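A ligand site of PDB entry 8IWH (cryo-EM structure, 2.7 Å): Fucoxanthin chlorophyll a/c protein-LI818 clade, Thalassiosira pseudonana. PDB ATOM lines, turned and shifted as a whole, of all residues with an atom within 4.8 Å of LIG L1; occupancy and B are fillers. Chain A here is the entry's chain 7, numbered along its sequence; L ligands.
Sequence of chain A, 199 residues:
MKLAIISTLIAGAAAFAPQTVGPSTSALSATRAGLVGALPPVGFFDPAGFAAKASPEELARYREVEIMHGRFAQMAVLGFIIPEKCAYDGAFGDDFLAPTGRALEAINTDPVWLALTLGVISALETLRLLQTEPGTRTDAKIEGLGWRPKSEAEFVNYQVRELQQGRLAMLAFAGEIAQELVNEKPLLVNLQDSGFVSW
The backbone carbonyl oxygen (O) of Val 65 sits at hydrogen-bond distance from a ring nitrogen (ND1) of His 69 (3.3 Å).
Tyr 62 touches LIG L1 (CE1 to O1, 3.1 Å).
Hydrophobic or aromatic side chains within 4 Å of LIG L1: Tyr 62 and His 69.
A magnesium atom (MG1) of LIG L1 is bound by a ring nitrogen (NE2) of His 69, 1.9 Å away.
The guanidinium group (NH1) of Arg 61 lies within salt-bridge range of an oxygen (O3) of LIG L1.
A ring nitrogen (ND1) of His 69 lies within hydrogen-bond range of an oxygen (O1) of LG4 L4 (3.0 Å).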
ATOM      1  N   ARG A  61      22.845 -21.340  18.733  1.00  0.00           N
ATOM      2  CA  ARG A  61      22.945 -22.641  18.083  1.00  0.00           C
ATOM      3  C   ARG A  61      22.142 -22.676  16.789  1.00  0.00           C
ATOM      4  O   ARG A  61      22.585 -23.241  15.790  1.00  0.00           O
ATOM      5  CB  ARG A  61      22.494 -23.736  19.040  1.00  0.00           C
ATOM      6  CG  ARG A  61      22.554 -25.143  18.474  1.00  0.00           C
ATOM      7  CD  ARG A  61      22.173 -26.160  19.530  1.00  0.00           C
ATOM      8  NE  ARG A  61      22.194 -27.512  19.014  1.00  0.00           N
ATOM      9  CZ  ARG A  61      21.145 -28.121  18.477  1.00  0.00           C
ATOM     10  NH1 ARG A  61      19.982 -27.517  18.366  1.00  0.00           N
ATOM     11  NH2 ARG A  61      21.277 -29.371  18.044  1.00  0.00           N
ATOM     12  N   TYR A  62      20.943 -22.094  16.804  1.00  0.00           N
ATOM     13  CA  TYR A  62      20.122 -22.051  15.600  1.00  0.00           C
ATOM     14  C   TYR A  62      20.823 -21.277  14.490  1.00  0.00           C
ATOM     15  O   TYR A  62      20.820 -21.696  13.327  1.00  0.00           O
ATOM     16  CB  TYR A  62      18.758 -21.429  15.890  1.00  0.00           C
ATOM     17  CG  TYR A  62      17.923 -22.198  16.892  1.00  0.00           C
ATOM     18  CD1 TYR A  62      18.172 -23.537  17.163  1.00  0.00           C
ATOM     19  CD2 TYR A  62      16.877 -21.586  17.558  1.00  0.00           C
ATOM     20  CE1 TYR A  62      17.409 -24.228  18.078  1.00  0.00           C
ATOM     21  CE2 TYR A  62      16.104 -22.274  18.474  1.00  0.00           C
ATOM     22  CZ  TYR A  62      16.371 -23.594  18.727  1.00  0.00           C
ATOM     23  OH  TYR A  62      15.608 -24.284  19.628  1.00  0.00           O
ATOM     24  N   VAL A  65      23.659 -23.393  13.085  1.00  0.00           N
ATOM     25  CA  VAL A  65      23.135 -24.479  12.259  1.00  0.00           C
ATOM     26  C   VAL A  65      22.687 -23.939  10.905  1.00  0.00           C
ATOM     27  O   VAL A  65      22.934 -24.554   9.866  1.00  0.00           O
ATOM     28  CB  VAL A  65      21.992 -25.203  12.983  1.00  0.00           C
ATOM     29  CG1 VAL A  65      21.149 -25.996  12.004  1.00  0.00           C
ATOM     30  CG2 VAL A  65      22.544 -26.114  14.065  1.00  0.00           C
ATOM     31  N   HIS A  69      24.359 -25.243   7.390  1.00  0.00           N
ATOM     32  CA  HIS A  69      23.478 -25.838   6.392  1.00  0.00           C
ATOM     33  C   HIS A  69      23.528 -25.045   5.094  1.00  0.00           C
ATOM     34  O   HIS A  69      23.567 -25.633   4.005  1.00  0.00           O
ATOM     35  CB  HIS A  69      22.050 -25.922   6.933  1.00  0.00           C
ATOM     36  CG  HIS A  69      21.721 -27.192   7.657  1.00  0.00           C
ATOM     37  ND1 HIS A  69      22.374 -27.605   8.798  1.00  0.00           N
ATOM     38  CD2 HIS A  69      20.766 -28.132   7.419  1.00  0.00           C
ATOM     39  CE1 HIS A  69      21.857 -28.743   9.210  1.00  0.00           C
ATOM     40  NE2 HIS A  69      20.873 -29.086   8.400  1.00  0.00           N
HETATM   41  N1  LIG L   1      18.174 -30.434   7.867  1.00  0.00           N
HETATM   42  N2  LIG L   1      21.205 -31.211  10.195  1.00  0.00           N
HETATM   43  C1  LIG L   1      19.143 -29.881  11.932  1.00  0.00           C
HETATM   44  C2  LIG L   1      16.993 -29.935   8.291  1.00  0.00           C
HETATM   45  C3  LIG L   1      20.153 -31.974   6.210  1.00  0.00           C
HETATM   46  C4  LIG L   1      22.297 -31.971   9.936  1.00  0.00           C
HETATM   47  C5  LIG L   1      18.034 -29.384  12.743  1.00  0.00           C
HETATM   48  C6  LIG L   1      16.018 -29.995   7.254  1.00  0.00           C
HETATM   49  C7  LIG L   1      21.021 -32.829   5.502  1.00  0.00           C
HETATM   50  C8  LIG L   1      22.995 -32.180  11.139  1.00  0.00           C
HETATM   51  C9  LIG L   1      16.999 -29.165  11.865  1.00  0.00           C
HETATM   52  C10 LIG L   1      16.635 -30.551   6.181  1.00  0.00           C
HETATM   53  C11 LIG L   1      22.071 -33.138   6.323  1.00  0.00           C
HETATM   54  C12 LIG L   1      22.307 -31.526  12.133  1.00  0.00           C
HETATM   55  C13 LIG L   1      17.445 -29.507  10.594  1.00  0.00           C
HETATM   56  C14 LIG L   1      17.986 -30.818   6.592  1.00  0.00           C
HETATM   57  C15 LIG L   1      21.793 -32.411   7.558  1.00  0.00           C
HETATM   58  C16 LIG L   1      21.201 -30.931  11.514  1.00  0.00           C
HETATM   59  C17 LIG L   1      17.995 -29.150  14.190  1.00  0.00           C
HETATM   60  C18 LIG L   1      16.026 -30.820   4.868  1.00  0.00           C
HETATM   61  C19 LIG L   1      23.230 -33.994   6.042  1.00  0.00           C
HETATM   62  C20 LIG L   1      22.283 -31.203  13.566  1.00  0.00           C
HETATM   63  C21 LIG L   1      17.907 -27.909  14.701  1.00  0.00           C
HETATM   64  C22 LIG L   1      15.718 -32.068   4.513  1.00  0.00           C
HETATM   65  C23 LIG L   1      24.074 -33.699   5.066  1.00  0.00           C
HETATM   66  C24 LIG L   1      20.935 -30.556  13.760  1.00  0.00           C
HETATM   67  C25 LIG L   1      19.342 -32.647  16.465  1.00  0.00           C
HETATM   68  C26 LIG L   1      17.428 -27.755  16.021  1.00  0.00           C
HETATM   69  C27 LIG L   1      20.047 -31.529  14.492  1.00  0.00           C
HETATM   70  C28 LIG L   1      20.415 -30.240  12.391  1.00  0.00           C
HETATM   71  C29 LIG L   1      16.622 -29.402   9.486  1.00  0.00           C
HETATM   72  C30 LIG L   1      18.907 -31.439   5.650  1.00  0.00           C
HETATM   73  C31 LIG L   1      22.759 -32.539   8.672  1.00  0.00           C
HETATM   74  C32 LIG L   1      15.623 -28.655  12.208  1.00  0.00           C
HETATM   75  C33 LIG L   1      14.590 -29.528   7.332  1.00  0.00           C
HETATM   76  C34 LIG L   1      20.804 -33.319   4.095  1.00  0.00           C
HETATM   77  C35 LIG L   1      24.265 -32.978  11.306  1.00  0.00           C
HETATM   78  N3  LIG L   1      18.746 -29.951  10.603  1.00  0.00           N
HETATM   79  N4  LIG L   1      20.632 -31.726   7.468  1.00  0.00           N
HETATM   80  O1  LIG L   1      16.929 -26.698  16.352  1.00  0.00           O
HETATM   81  O2  LIG L   1      19.430 -32.368  13.868  1.00  0.00           O
HETATM   82  O3  LIG L   1      17.253 -28.843  16.797  1.00  0.00           O
HETATM   83  O4  LIG L   1      20.033 -31.536  15.830  1.00  0.00           O
HETATM   84  O5  LIG L   1      23.017 -31.650  14.432  1.00  0.00           O
HETATM   85 MG1  LIG L   1      19.820 -30.565   8.949  1.00  0.00          MG
HETATM   86  C1  LG2 L   2      13.917 -24.566   6.628  1.00  0.00           C
HETATM   87  C2  LG2 L   2      14.796 -25.312   5.658  1.00  0.00           C
HETATM   88  C3  LG2 L   2      15.450 -26.498   5.846  1.00  0.00           C
HETATM   89  C4  LG2 L   2      16.335 -27.194   4.791  1.00  0.00           C
HETATM   90  C5  LG2 L   2      17.588 -27.707   5.061  1.00  0.00           C
HETATM   91  C6  LG2 L   2      18.503 -28.390   4.087  1.00  0.00           C
HETATM   92  C7  LG2 L   2      21.857 -29.503   2.758  1.00  0.00           C
HETATM   93  C8  LG2 L   2      20.573 -29.012   2.700  1.00  0.00           C
HETATM   94  C9  LG2 L   2      19.823 -28.225   3.750  1.00  0.00           C
HETATM   95  C10 LG2 L   2       9.753 -22.236   9.661  1.00  0.00           C
HETATM   96  C11 LG2 L   2       9.259 -21.789  11.077  1.00  0.00           C
HETATM   97  C12 LG2 L   2       9.796 -20.429  11.618  1.00  0.00           C
HETATM   98  C13 LG2 L   2      10.802 -19.765  10.581  1.00  0.00           C
HETATM   99  C14 LG2 L   2      11.767 -20.757   9.931  1.00  0.00           C
HETATM  100  C15 LG2 L   2      11.297 -21.971   9.508  1.00  0.00           C
HETATM  101  C16 LG2 L   2      12.201 -22.716   8.603  1.00  0.00           C
HETATM  102  C17 LG2 L   2      11.877 -23.129   7.243  1.00  0.00           C
HETATM  103  C18 LG2 L   2      12.784 -23.911   6.275  1.00  0.00           C
HETATM  104  C19 LG2 L   2      22.575 -30.304   1.641  1.00  0.00           C
HETATM  105  C20 LG2 L   2      23.578 -31.213   1.707  1.00  0.00           C
HETATM  106  C21 LG2 L   2      24.187 -31.958   0.525  1.00  0.00           C
HETATM  107  C22 LG2 L   2      25.409 -32.572   0.363  1.00  0.00           C
HETATM  108  C23 LG2 L   2      25.766 -33.235  -0.903  1.00  0.00           C
HETATM  109  C24 LG2 L   2      13.104 -20.219   9.417  1.00  0.00           C
HETATM  110  C25 LG2 L   2       8.924 -21.570   8.557  1.00  0.00           C
HETATM  111  C26 LG2 L   2       9.543 -23.772   9.528  1.00  0.00           C
HETATM  112  C27 LG2 L   2      12.410 -23.988   4.796  1.00  0.00           C
HETATM  113  C28 LG2 L   2      15.810 -27.326   3.372  1.00  0.00           C
HETATM  114  C29 LG2 L   2      26.255 -32.455   1.614  1.00  0.00           C
HETATM  115  C30 LG2 L   2      22.623 -29.216   4.035  1.00  0.00           C
HETATM  116  C31 LG2 L   2      26.056 -33.797  -1.954  1.00  0.00           C
HETATM  117  C32 LG2 L   2      26.388 -34.473  -3.166  1.00  0.00           C
HETATM  118  C33 LG2 L   2      25.882 -35.891  -3.257  1.00  0.00           C
HETATM  119  C34 LG2 L   2      26.476 -36.762  -4.338  1.00  0.00           C
HETATM  120  C35 LG2 L   2      26.566 -35.954  -5.597  1.00  0.00           C
HETATM  121  C36 LG2 L   2      27.527 -34.797  -5.282  1.00  0.00           C
HETATM  122  C37 LG2 L   2      27.102 -33.914  -4.189  1.00  0.00           C
HETATM  123  C38 LG2 L   2      27.313 -32.461  -4.448  1.00  0.00           C
HETATM  124  C39 LG2 L   2      26.165 -36.614  -1.964  1.00  0.00           C
HETATM  125  C40 LG2 L   2      24.370 -35.792  -3.554  1.00  0.00           C
HETATM  126  O1  LG2 L   2       8.694 -19.595  11.932  1.00  0.00           O
HETATM  127  O2  LG2 L   2      27.005 -36.617  -6.740  1.00  0.00           O
HETATM  128 MG1  LG3 L   3      15.745 -19.235   8.968  1.00  0.00          MG
HETATM  129  C1  LG3 L   3      15.163 -16.297  10.714  1.00  0.00           C
HETATM  130  C2  LG3 L   3      17.115 -20.617  11.737  1.00  0.00           C
HETATM  131  C3  LG3 L   3      16.232 -22.136   7.191  1.00  0.00           C
HETATM  132  C4  LG3 L   3      14.204 -17.785   6.136  1.00  0.00           C
HETATM  133  N1  LG3 L   3      16.085 -18.536  10.904  1.00  0.00           N
HETATM  134  C5  LG3 L   3      15.763 -17.286  11.448  1.00  0.00           C
HETATM  135  C6  LG3 L   3      16.184 -17.202  12.908  1.00  0.00           C
HETATM  136  C7  LG3 L   3      16.850 -18.578  13.181  1.00  0.00           C
HETATM  137  C8  LG3 L   3      16.687 -19.314  11.858  1.00  0.00           C
HETATM  138  C9  LG3 L   3      18.299 -18.424  13.567  1.00  0.00           C
HETATM  139  C10 LG3 L   3      14.972 -17.040  13.801  1.00  0.00           C
HETATM  140  C11 LG3 L   3      13.908 -18.048  13.457  1.00  0.00           C
HETATM  141  C12 LG3 L   3      13.579 -18.877  14.659  1.00  0.00           C
HETATM  142  O1  LG3 L   3      13.029 -18.524  15.708  1.00  0.00           O
HETATM  143  O2  LG3 L   3      13.951 -20.189  14.550  1.00  0.00           O
HETATM  144  N2  LG3 L   3      16.525 -21.032   9.383  1.00  0.00           N
HETATM  145  C13 LG3 L   3      17.034 -21.409  10.586  1.00  0.00           C
HETATM  146  C14 LG3 L   3      17.520 -22.814  10.514  1.00  0.00           C
HETATM  147  C15 LG3 L   3      17.274 -23.256   9.222  1.00  0.00           C
HETATM  148  C16 LG3 L   3      16.647 -22.123   8.489  1.00  0.00           C
HETATM  149  C17 LG3 L   3      18.128 -23.494  11.648  1.00  0.00           C
HETATM  150  C18 LG3 L   3      17.532 -24.520   8.596  1.00  0.00           C
HETATM  151  C19 LG3 L   3      17.462 -25.724   9.191  1.00  0.00           C
HETATM  152  N3  LG3 L   3      15.313 -19.837   7.010  1.00  0.00           N
HETATM  153  C20 LG3 L   3      15.612 -21.067   6.498  1.00  0.00           C
HETATM  154  C21 LG3 L   3      15.169 -21.138   5.111  1.00  0.00           C
HETATM  155  C22 LG3 L   3      14.570 -19.932   4.805  1.00  0.00           C
HETATM  156  C23 LG3 L   3      14.658 -19.105   6.005  1.00  0.00           C
HETATM  157  C24 LG3 L   3      15.326 -22.302   4.241  1.00  0.00           C
HETATM  158  C25 LG3 L   3      13.940 -19.576   3.519  1.00  0.00           C
HETATM  159  C26 LG3 L   3      14.562 -18.389   2.831  1.00  0.00           C
HETATM  160  N4  LG3 L   3      14.916 -17.464   8.462  1.00  0.00           N
HETATM  161  C27 LG3 L   3      14.313 -17.000   7.258  1.00  0.00           C
HETATM  162  C28 LG3 L   3      13.870 -15.610   7.450  1.00  0.00           C
HETATM  163  C29 LG3 L   3      14.181 -15.275   8.754  1.00  0.00           C
HETATM  164  C30 LG3 L   3      14.805 -16.477   9.348  1.00  0.00           C
HETATM  165  C31 LG3 L   3      13.239 -14.790   6.416  1.00  0.00           C
HETATM  166  C32 LG3 L   3      14.146 -14.250   9.776  1.00  0.00           C
HETATM  167  O3  LG3 L   3      13.741 -13.101   9.694  1.00  0.00           O
HETATM  168  C33 LG3 L   3      14.736 -14.886  11.075  1.00  0.00           C
HETATM  169  C34 LG3 L   3      15.872 -14.072  11.646  1.00  0.00           C
HETATM  170  O4  LG3 L   3      16.508 -14.278  12.670  1.00  0.00           O
HETATM  171  O5  LG3 L   3      16.187 -12.967  10.925  1.00  0.00           O
HETATM  172  C35 LG3 L   3      16.309 -11.741  11.652  1.00  0.00           C
HETATM  173  C36 LG3 L   3      13.877 -20.787  13.243  1.00  0.00           C
HETATM  174  C37 LG3 L   3      13.501 -22.210  13.411  1.00  0.00           C
HETATM  175  C38 LG3 L   3      14.335 -23.153  13.877  1.00  0.00           C
HETATM  176  C39 LG3 L   3      15.726 -22.854  14.286  1.00  0.00           C
HETATM  177  C40 LG3 L   3      13.886 -24.564  14.025  1.00  0.00           C
HETATM  178  C41 LG3 L   3      13.942 -25.350  12.726  1.00  0.00           C
HETATM  179  C42 LG3 L   3      12.611 -25.313  12.014  1.00  0.00           C
HETATM  180  C43 LG3 L   3      11.947 -26.689  11.884  1.00  0.00           C
HETATM  181  C44 LG3 L   3      12.237 -27.591  13.070  1.00  0.00           C
HETATM  182  C45 LG3 L   3      12.360 -27.370  10.587  1.00  0.00           C
HETATM  183  C46 LG3 L   3      11.149 -27.848   9.817  1.00  0.00           C
HETATM  184  C47 LG3 L   3      11.224 -27.443   8.357  1.00  0.00           C
HETATM  185  C48 LG3 L   3      10.037 -27.967   7.573  1.00  0.00           C
HETATM  186  C49 LG3 L   3      10.100 -29.471   7.442  1.00  0.00           C
HETATM  187  C50 LG3 L   3       9.913 -27.270   6.221  1.00  0.00           C
HETATM  188  C51 LG3 L   3      10.376 -28.136   5.067  1.00  0.00           C
HETATM  189  C52 LG3 L   3      10.658 -27.312   3.835  1.00  0.00           C
HETATM  190  C53 LG3 L   3      10.727 -28.145   2.551  1.00  0.00           C
HETATM  191  C54 LG3 L   3      11.434 -27.385   1.460  1.00  0.00           C
HETATM  192  C55 LG3 L   3      11.413 -29.471   2.796  1.00  0.00           C
HETATM  193 MG1  LG4 L   4      28.968 -32.508  10.855  1.00  0.00          MG
HETATM  194  C1  LG4 L   4      27.195 -29.828  12.138  1.00  0.00           C
HETATM  195  C2  LG4 L   4      30.472 -32.948  13.876  1.00  0.00           C
HETATM  196  C3  LG4 L   4      30.416 -35.383   9.656  1.00  0.00           C
HETATM  197  C4  LG4 L   4      27.278 -32.096   7.776  1.00  0.00           C
HETATM  198  N1  LG4 L   4      28.882 -31.492  12.669  1.00  0.00           N
HETATM  199  C5  LG4 L   4      28.068 -30.412  13.013  1.00  0.00           C
HETATM  200  C6  LG4 L   4      28.308 -29.976  14.447  1.00  0.00           C
HETATM  201  C7  LG4 L   4      29.511 -30.838  14.889  1.00  0.00           C
HETATM  202  C8  LG4 L   4      29.644 -31.847  13.750  1.00  0.00           C
HETATM  203  C9  LG4 L   4      30.752 -30.011  15.071  1.00  0.00           C
HETATM  204  C10 LG4 L   4      27.087 -30.277  15.301  1.00  0.00           C
HETATM  205  N2  LG4 L   4      30.281 -33.846  11.589  1.00  0.00           N
HETATM  206  C11 LG4 L   4      30.666 -33.930  12.885  1.00  0.00           C
HETATM  207  C12 LG4 L   4      31.345 -35.222  13.136  1.00  0.00           C
HETATM  208  C13 LG4 L   4      31.334 -35.921  11.950  1.00  0.00           C
HETATM  209  C14 LG4 L   4      30.648 -35.053  10.952  1.00  0.00           C
HETATM  210  C15 LG4 L   4      31.876 -35.609  14.437  1.00  0.00           C
HETATM  211  C16 LG4 L   4      31.828 -37.225  11.622  1.00  0.00           C
HETATM  212  C17 LG4 L   4      31.583 -38.339  12.314  1.00  0.00           C
HETATM  213  N3  LG4 L   4      28.921 -33.503   9.020  1.00  0.00           N
HETATM  214  C18 LG4 L   4      29.601 -34.653   8.741  1.00  0.00           C
HETATM  215  C19 LG4 L   4      29.340 -35.069   7.374  1.00  0.00           C
HETATM  216  C20 LG4 L   4      28.422 -34.166   6.850  1.00  0.00           C
HETATM  217  C21 LG4 L   4      28.165 -33.183   7.897  1.00  0.00           C
HETATM  218  C22 LG4 L   4      29.922 -36.259   6.744  1.00  0.00           C
HETATM  219  C23 LG4 L   4      27.842 -34.179   5.506  1.00  0.00           C
HETATM  220  C24 LG4 L   4      28.780 -33.625   4.465  1.00  0.00           C
HETATM  221  N4  LG4 L   4      27.610 -31.248  10.050  1.00  0.00           N
HETATM  222  C25 LG4 L   4      27.001 -31.182   8.775  1.00  0.00           C
HETATM  223  C26 LG4 L   4      26.064 -30.043   8.747  1.00  0.00           C
HETATM  224  C27 LG4 L   4      26.095 -29.489  10.010  1.00  0.00           C
HETATM  225  C28 LG4 L   4      27.072 -30.281  10.789  1.00  0.00           C
HETATM  226  C29 LG4 L   4      25.272 -29.647   7.586  1.00  0.00           C
HETATM  227  C30 LG4 L   4      25.592 -28.452  10.889  1.00  0.00           C
HETATM  228  O1  LG4 L   4      24.794 -27.554  10.653  1.00  0.00           O
HETATM  229  C31 LG4 L   4      26.261 -28.648  12.281  1.00  0.00           C
HETATM  230  C32 LG4 L   4      27.024 -27.437  12.723  1.00  0.00           C
HETATM  231  O2  LG4 L   4      28.213 -27.188  12.547  1.00  0.00           O
HETATM  232  O3  LG4 L   4      26.273 -26.532  13.398  1.00  0.00           O
HETATM  233  C33 LG4 L   4      26.450 -26.455  14.817  1.00  0.00           C
